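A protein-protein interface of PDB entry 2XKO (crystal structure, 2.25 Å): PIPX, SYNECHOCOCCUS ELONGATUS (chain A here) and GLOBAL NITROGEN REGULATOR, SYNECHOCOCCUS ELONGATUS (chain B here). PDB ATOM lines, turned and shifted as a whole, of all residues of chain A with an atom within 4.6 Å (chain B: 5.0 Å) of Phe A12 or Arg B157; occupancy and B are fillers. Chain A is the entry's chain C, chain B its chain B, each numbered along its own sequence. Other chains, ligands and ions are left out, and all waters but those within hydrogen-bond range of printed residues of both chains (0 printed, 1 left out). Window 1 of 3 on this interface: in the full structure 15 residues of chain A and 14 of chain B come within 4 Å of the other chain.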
ATOM      1  N   ASN A   8      -7.032  11.922 -19.302  1.00  0.00           N
ATOM      2  CA  ASN A   8      -5.690  12.060 -19.846  1.00  0.00           C
ATOM      3  C   ASN A   8      -5.556  11.327 -21.153  1.00  0.00           C
ATOM      4  O   ASN A   8      -5.618  10.111 -21.173  1.00  0.00           O
ATOM      5  CB  ASN A   8      -4.656  11.518 -18.851  1.00  0.00           C
ATOM      6  CG  ASN A   8      -3.583  12.537 -18.511  1.00  0.00           C
ATOM      7  OD1 ASN A   8      -3.468  13.579 -19.163  1.00  0.00           O
ATOM      8  ND2 ASN A   8      -2.813  12.255 -17.457  1.00  0.00           N
ATOM      9  N   HIS A   9      -5.398  12.069 -22.243  1.00  0.00           N
ATOM     10  CA  HIS A   9      -5.024  11.490 -23.540  1.00  0.00           C
ATOM     11  C   HIS A   9      -3.516  11.195 -23.520  1.00  0.00           C
ATOM     12  O   HIS A   9      -2.732  12.052 -23.110  1.00  0.00           O
ATOM     13  CB  HIS A   9      -5.360  12.483 -24.650  1.00  0.00           C
ATOM     14  CG  HIS A   9      -5.272  11.923 -26.033  1.00  0.00           C
ATOM     15  ND1 HIS A   9      -4.129  11.335 -26.528  1.00  0.00           N
ATOM     16  CD2 HIS A   9      -6.163  11.930 -27.053  1.00  0.00           C
ATOM     17  CE1 HIS A   9      -4.327  10.969 -27.781  1.00  0.00           C
ATOM     18  NE2 HIS A   9      -5.554  11.320 -28.126  1.00  0.00           N
ATOM     19  N   PRO A  10      -3.098   9.982 -23.955  1.00  0.00           N
ATOM     20  CA  PRO A  10      -1.673   9.585 -23.899  1.00  0.00           C
ATOM     21  C   PRO A  10      -0.731  10.524 -24.636  1.00  0.00           C
ATOM     22  O   PRO A  10       0.415  10.700 -24.236  1.00  0.00           O
ATOM     23  CB  PRO A  10      -1.640   8.213 -24.586  1.00  0.00           C
ATOM     24  CG  PRO A  10      -3.030   7.828 -24.850  1.00  0.00           C
ATOM     25  CD  PRO A  10      -3.962   8.925 -24.505  1.00  0.00           C
ATOM     26  N   THR A  11      -1.217  11.083 -25.733  1.00  0.00           N
ATOM     27  CA  THR A  11      -0.451  12.014 -26.523  1.00  0.00           C
ATOM     28  C   THR A  11      -0.736  13.448 -26.138  1.00  0.00           C
ATOM     29  O   THR A  11       0.202  14.220 -25.968  1.00  0.00           O
ATOM     30  CB  THR A  11      -0.756  11.864 -28.022  1.00  0.00           C
ATOM     31  OG1 THR A  11      -0.586  10.499 -28.399  1.00  0.00           O
ATOM     32  CG2 THR A  11       0.179  12.757 -28.849  1.00  0.00           C
ATOM     33  N   PHE A  12      -2.017  13.810 -26.005  1.00  0.00           N
ATOM     34  CA  PHE A  12      -2.398  15.238 -25.942  1.00  0.00           C
ATOM     35  C   PHE A  12      -2.507  15.831 -24.547  1.00  0.00           C
ATOM     36  O   PHE A  12      -2.687  17.036 -24.402  1.00  0.00           O
ATOM     37  CB  PHE A  12      -3.686  15.485 -26.725  1.00  0.00           C
ATOM     38  CG  PHE A  12      -3.514  15.373 -28.216  1.00  0.00           C
ATOM     39  CD1 PHE A  12      -2.958  16.413 -28.942  1.00  0.00           C
ATOM     40  CD2 PHE A  12      -3.882  14.214 -28.882  1.00  0.00           C
ATOM     41  CE1 PHE A  12      -2.787  16.299 -30.311  1.00  0.00           C
ATOM     42  CE2 PHE A  12      -3.718  14.086 -30.255  1.00  0.00           C
ATOM     43  CZ  PHE A  12      -3.174  15.126 -30.972  1.00  0.00           C
ATOM     44  N   GLY A  13      -2.371  14.999 -23.530  1.00  0.00           N
ATOM     45  CA  GLY A  13      -2.454  15.464 -22.143  1.00  0.00           C
ATOM     46  C   GLY A  13      -3.884  15.621 -21.659  1.00  0.00           C
ATOM     47  O   GLY A  13      -4.802  15.000 -22.189  1.00  0.00           O
ATOM     48  N   LEU A  14      -4.070  16.479 -20.656  1.00  0.00           N
ATOM     49  CA  LEU A  14      -5.351  16.583 -19.952  1.00  0.00           C
ATOM     50  C   LEU A  14      -6.459  17.116 -20.860  1.00  0.00           C
ATOM     51  O   LEU A  14      -6.300  18.120 -21.560  1.00  0.00           O
ATOM     52  CB  LEU A  14      -5.193  17.476 -18.719  1.00  0.00           C
ATOM     53  CG  LEU A  14      -6.097  17.209 -17.524  1.00  0.00           C
ATOM     54  CD1 LEU A  14      -5.949  15.783 -17.012  1.00  0.00           C
ATOM     55  CD2 LEU A  14      -5.755  18.209 -16.449  1.00  0.00           C
ATOM     56  N   LEU A  15      -7.581  16.412 -20.864  1.00  0.00           N
ATOM     57  CA  LEU A  15      -8.767  16.845 -21.605  1.00  0.00           C
ATOM     58  C   LEU A  15      -9.884  17.099 -20.601  1.00  0.00           C
ATOM     59  O   LEU A  15      -9.828  16.584 -19.485  1.00  0.00           O
ATOM     60  CB  LEU A  15      -9.169  15.767 -22.596  1.00  0.00           C
ATOM     61  CG  LEU A  15      -8.059  15.246 -23.523  1.00  0.00           C
ATOM     62  CD1 LEU A  15      -8.595  14.049 -24.311  1.00  0.00           C
ATOM     63  CD2 LEU A  15      -7.522  16.342 -24.466  1.00  0.00           C
ATOM     64  N   LEU A  31      -7.409  21.213 -22.931  1.00  0.00           N
ATOM     65  CA  LEU A  31      -7.457  22.214 -21.879  1.00  0.00           C
ATOM     66  C   LEU A  31      -7.018  23.567 -22.411  1.00  0.00           C
ATOM     67  O   LEU A  31      -7.639  24.576 -22.103  1.00  0.00           O
ATOM     68  CB  LEU A  31      -6.548  21.783 -20.732  1.00  0.00           C
ATOM     69  CG  LEU A  31      -6.908  22.290 -19.351  1.00  0.00           C
ATOM     70  CD1 LEU A  31      -8.239  21.677 -18.904  1.00  0.00           C
ATOM     71  CD2 LEU A  31      -5.803  21.923 -18.392  1.00  0.00           C
ATOM     72  N   LEU A  36      -8.248  21.210 -30.009  1.00  0.00           N
ATOM     73  CA  LEU A  36      -8.661  19.901 -30.468  1.00  0.00           C
ATOM     74  C   LEU A  36      -9.831  19.380 -29.618  1.00  0.00           C
ATOM     75  O   LEU A  36      -9.893  19.570 -28.380  1.00  0.00           O
ATOM     76  CB  LEU A  36      -7.504  18.912 -30.428  1.00  0.00           C
ATOM     77  CG  LEU A  36      -6.159  19.260 -31.093  1.00  0.00           C
ATOM     78  CD1 LEU A  36      -5.153  18.217 -30.677  1.00  0.00           C
ATOM     79  CD2 LEU A  36      -6.224  19.336 -32.628  1.00  0.00           C
ATOM     80  N   PHE A  38     -12.324  15.780 -29.117  1.00  0.00           N
ATOM     81  CA  PHE A  38     -12.259  14.327 -29.249  1.00  0.00           C
ATOM     82  C   PHE A  38     -13.562  13.657 -28.876  1.00  0.00           C
ATOM     83  O   PHE A  38     -14.055  13.851 -27.778  1.00  0.00           O
ATOM     84  CB  PHE A  38     -11.163  13.741 -28.348  1.00  0.00           C
ATOM     85  CG  PHE A  38      -9.796  14.150 -28.726  1.00  0.00           C
ATOM     86  CD1 PHE A  38      -9.080  13.433 -29.704  1.00  0.00           C
ATOM     87  CD2 PHE A  38      -9.193  15.243 -28.117  1.00  0.00           C
ATOM     88  CE1 PHE A  38      -7.785  13.811 -30.068  1.00  0.00           C
ATOM     89  CE2 PHE A  38      -7.904  15.629 -28.489  1.00  0.00           C
ATOM     90  CZ  PHE A  38      -7.202  14.904 -29.460  1.00  0.00           C
ATOM     91  N   ARG B  69       6.658  15.020 -20.642  1.00  0.00           N
ATOM     92  CA  ARG B  69       5.793  14.121 -19.906  1.00  0.00           C
ATOM     93  C   ARG B  69       5.886  12.695 -20.427  1.00  0.00           C
ATOM     94  O   ARG B  69       6.480  12.423 -21.452  1.00  0.00           O
ATOM     95  CB  ARG B  69       4.345  14.595 -19.983  1.00  0.00           C
ATOM     96  CG  ARG B  69       3.768  14.687 -21.386  1.00  0.00           C
ATOM     97  CD  ARG B  69       2.297  15.018 -21.349  1.00  0.00           C
ATOM     98  NE  ARG B  69       1.493  13.859 -21.693  1.00  0.00           N
ATOM     99  CZ  ARG B  69       0.544  13.308 -20.948  1.00  0.00           C
ATOM    100  NH1 ARG B  69       0.190  13.802 -19.763  1.00  0.00           N
ATOM    101  NH2 ARG B  69      -0.083  12.252 -21.423  1.00  0.00           N
ATOM    102  N   GLN B 131       4.493  20.593 -29.104  1.00  0.00           N
ATOM    103  CA  GLN B 131       4.779  21.008 -27.713  1.00  0.00           C
ATOM    104  C   GLN B 131       5.846  22.118 -27.634  1.00  0.00           C
ATOM    105  O   GLN B 131       5.674  23.102 -26.921  1.00  0.00           O
ATOM    106  CB  GLN B 131       5.225  19.812 -26.876  1.00  0.00           C
ATOM    107  CG  GLN B 131       4.154  18.693 -26.739  1.00  0.00           C
ATOM    108  CD  GLN B 131       4.690  17.453 -26.013  1.00  0.00           C
ATOM    109  OE1 GLN B 131       5.397  17.583 -25.026  1.00  0.00           O
ATOM    110  NE2 GLN B 131       4.362  16.257 -26.513  1.00  0.00           N
ATOM    111  N   MET B 134       4.397  25.395 -28.698  1.00  0.00           N
ATOM    112  CA  MET B 134       3.611  26.034 -27.644  1.00  0.00           C
ATOM    113  C   MET B 134       4.456  26.727 -26.608  1.00  0.00           C
ATOM    114  O   MET B 134       4.037  27.734 -26.086  1.00  0.00           O
ATOM    115  CB  MET B 134       2.633  25.061 -26.962  1.00  0.00           C
ATOM    116  CG  MET B 134       1.397  24.938 -27.785  1.00  0.00           C
ATOM    117  SD  MET B 134       0.229  23.701 -27.213  1.00  0.00           S
ATOM    118  CE  MET B 134      -0.464  24.572 -25.807  1.00  0.00           C
ATOM    119  N   LEU B 153      -0.583  26.892 -17.573  1.00  0.00           N
ATOM    120  CA  LEU B 153      -1.611  26.179 -18.375  1.00  0.00           C
ATOM    121  C   LEU B 153      -1.025  24.966 -19.115  1.00  0.00           C
ATOM    122  O   LEU B 153      -1.664  23.918 -19.202  1.00  0.00           O
ATOM    123  CB  LEU B 153      -2.259  27.146 -19.360  1.00  0.00           C
ATOM    124  CG  LEU B 153      -3.084  28.268 -18.696  1.00  0.00           C
ATOM    125  CD1 LEU B 153      -3.708  29.081 -19.792  1.00  0.00           C
ATOM    126  CD2 LEU B 153      -4.151  27.681 -17.691  1.00  0.00           C
ATOM    127  N   ILE B 154       0.208  25.095 -19.616  1.00  0.00           N
ATOM    128  CA  ILE B 154       0.919  23.958 -20.201  1.00  0.00           C
ATOM    129  C   ILE B 154       1.255  22.926 -19.134  1.00  0.00           C
ATOM    130  O   ILE B 154       1.111  21.744 -19.387  1.00  0.00           O
ATOM    131  CB  ILE B 154       2.165  24.376 -20.992  1.00  0.00           C
ATOM    132  CG1 ILE B 154       1.751  25.151 -22.260  1.00  0.00           C
ATOM    133  CG2 ILE B 154       2.989  23.161 -21.370  1.00  0.00           C
ATOM    134  CD1 ILE B 154       2.880  25.927 -22.927  1.00  0.00           C
ATOM    135  N   LEU B 155       1.676  23.330 -17.935  1.00  0.00           N
ATOM    136  CA  LEU B 155       1.918  22.329 -16.899  1.00  0.00           C
ATOM    137  C   LEU B 155       0.621  21.631 -16.502  1.00  0.00           C
ATOM    138  O   LEU B 155       0.636  20.415 -16.283  1.00  0.00           O
ATOM    139  CB  LEU B 155       2.640  22.916 -15.693  1.00  0.00           C
ATOM    140  CG  LEU B 155       4.059  23.460 -15.987  1.00  0.00           C
ATOM    141  CD1 LEU B 155       4.727  24.015 -14.732  1.00  0.00           C
ATOM    142  CD2 LEU B 155       4.972  22.386 -16.647  1.00  0.00           C
ATOM    143  N   CYS B 156      -0.505  22.361 -16.475  1.00  0.00           N
ATOM    144  CA  CYS B 156      -1.787  21.717 -16.194  1.00  0.00           C
ATOM    145  C   CYS B 156      -2.088  20.633 -17.243  1.00  0.00           C
ATOM    146  O   CYS B 156      -2.538  19.544 -16.901  1.00  0.00           O
ATOM    147  CB  CYS B 156      -2.955  22.722 -16.169  1.00  0.00           C
ATOM    148  SG  CYS B 156      -2.904  23.850 -14.840  1.00  0.00           S
ATOM    149  N   ARG B 157      -1.837  20.943 -18.509  1.00  0.00           N
ATOM    150  CA  ARG B 157      -2.079  19.990 -19.581  1.00  0.00           C
ATOM    151  C   ARG B 157      -1.183  18.759 -19.442  1.00  0.00           C
ATOM    152  O   ARG B 157      -1.627  17.647 -19.617  1.00  0.00           O
ATOM    153  CB  ARG B 157      -1.843  20.656 -20.935  1.00  0.00           C
ATOM    154  CG  ARG B 157      -1.838  19.695 -22.107  1.00  0.00           C
ATOM    155  CD  ARG B 157      -1.224  20.307 -23.338  1.00  0.00           C
ATOM    156  NE  ARG B 157       0.217  20.188 -23.325  1.00  0.00           N
ATOM    157  CZ  ARG B 157       1.029  20.856 -24.140  1.00  0.00           C
ATOM    158  NH1 ARG B 157       0.520  21.710 -25.026  1.00  0.00           N
ATOM    159  NH2 ARG B 157       2.362  20.697 -24.040  1.00  0.00           N
ATOM    160  N   ASP B 158       0.087  18.972 -19.132  1.00  0.00           N
ATOM    161  CA  ASP B 158       1.054  17.891 -19.168  1.00  0.00           C
ATOM    162  C   ASP B 158       1.102  17.104 -17.877  1.00  0.00           C
ATOM    163  O   ASP B 158       1.285  15.868 -17.920  1.00  0.00           O
ATOM    164  CB  ASP B 158       2.453  18.437 -19.501  1.00  0.00           C
ATOM    165  CG  ASP B 158       2.594  18.811 -20.969  1.00  0.00           C
ATOM    166  OD1 ASP B 158       1.741  18.389 -21.788  1.00  0.00           O
ATOM    167  OD2 ASP B 158       3.558  19.519 -21.303  1.00  0.00           O
ATOM    168  N   PHE B 159       0.956  17.801 -16.740  1.00  0.00           N
ATOM    169  CA  PHE B 159       1.176  17.208 -15.436  1.00  0.00           C
ATOM    170  C   PHE B 159       0.038  17.424 -14.439  1.00  0.00           C
ATOM    171  O   PHE B 159       0.203  17.119 -13.267  1.00  0.00           O
ATOM    172  CB  PHE B 159       2.452  17.786 -14.815  1.00  0.00           C
ATOM    173  CG  PHE B 159       3.639  17.629 -15.668  1.00  0.00           C
ATOM    174  CD1 PHE B 159       4.302  16.409 -15.736  1.00  0.00           C
ATOM    175  CD2 PHE B 159       4.088  18.678 -16.460  1.00  0.00           C
ATOM    176  CE1 PHE B 159       5.423  16.245 -16.591  1.00  0.00           C
ATOM    177  CE2 PHE B 159       5.213  18.517 -17.302  1.00  0.00           C
ATOM    178  CZ  PHE B 159       5.866  17.316 -17.369  1.00  0.00           C
ATOM    179  N   GLY B 160      -1.107  17.918 -14.883  1.00  0.00           N
ATOM    180  CA  GLY B 160      -2.172  18.297 -13.959  1.00  0.00           C
ATOM    181  C   GLY B 160      -3.011  17.147 -13.447  1.00  0.00           C
ATOM    182  O   GLY B 160      -3.166  16.169 -14.150  1.00  0.00           O
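Printed residues of chain A that touch a printed residue of chain B: Asn A8, His A9, Pro A10, Phe A12, Gly A13, Leu A14 and Leu A31.
Hydrophobic or aromatic side chains of chain A that line the printed part of chain B: Leu A14 and Leu A31.
Of the 11 printed residues of chain B, 3 touch a printed residue of chain A.
Printed residues of chain B that touch a printed residue of chain A: Arg B69, Cys B156 and Arg B157.
Of the printed residues of chain B, Asn A8 touches Arg B69.
Printed residues of chain B within 4 Å of Leu A31: Cys B156 (3.7 Å).
Leu A36 touches none of the printed residues of chain B.
Of chain A, only Phe A12, Gly A13 and Leu A14 come within 4 Å of Arg B157.
Asp B158 touches none of the printed residues of chain A.
The nearest printed residue of chain B that does not touch Leu A14 is Gly B160 (4.01 Å).
O of His A9 is in hydrogen-bond range of NH2 of Arg B69.
NH2 of Arg B69 lies within hydrogen-bond range of O of Pro A10 (3.3 Å).
The backbone NH of Leu A14 lies within hydrogen-bond range of the backbone carbonyl oxygen of Arg B157, at 2.9 Å.
The guanidinium group of Arg B69 lies within hydrogen-bond range of the backbone carbonyl oxygen of Asp B158 (3.0 Å).
SD of Met B134 is in hydrogen-bond range of NH1 of Arg B157 (3.0 Å).
ND1 of His A9 is in hydrogen-bond range of N of Phe A12 (3.3 Å).
ND1 of His A9 is in hydrogen-bond range of N of Thr A11.
The guanidinium group (NE) of Arg B157 is in salt-bridge range of the side-chain carboxylate (OD1) of Asp B158, at 2.8 Å.
OD1 of Asn A8 sits at hydrogen-bond distance from N of Leu A14, at 3.3 Å.
Arg B69 touches Asn A8 (NH1 to OD1, 3.7 Å).
O of Phe A12 touches CG of Arg B157, 3.6 Å away.
Gly A13 touches Arg B69.
Arg B157 touches Gly A13.
O of Cys B156 touches CD2 of Leu A14 (3.5 Å).
Cys B156 touches Leu A31 (CB to CD2, 3.7 Å).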
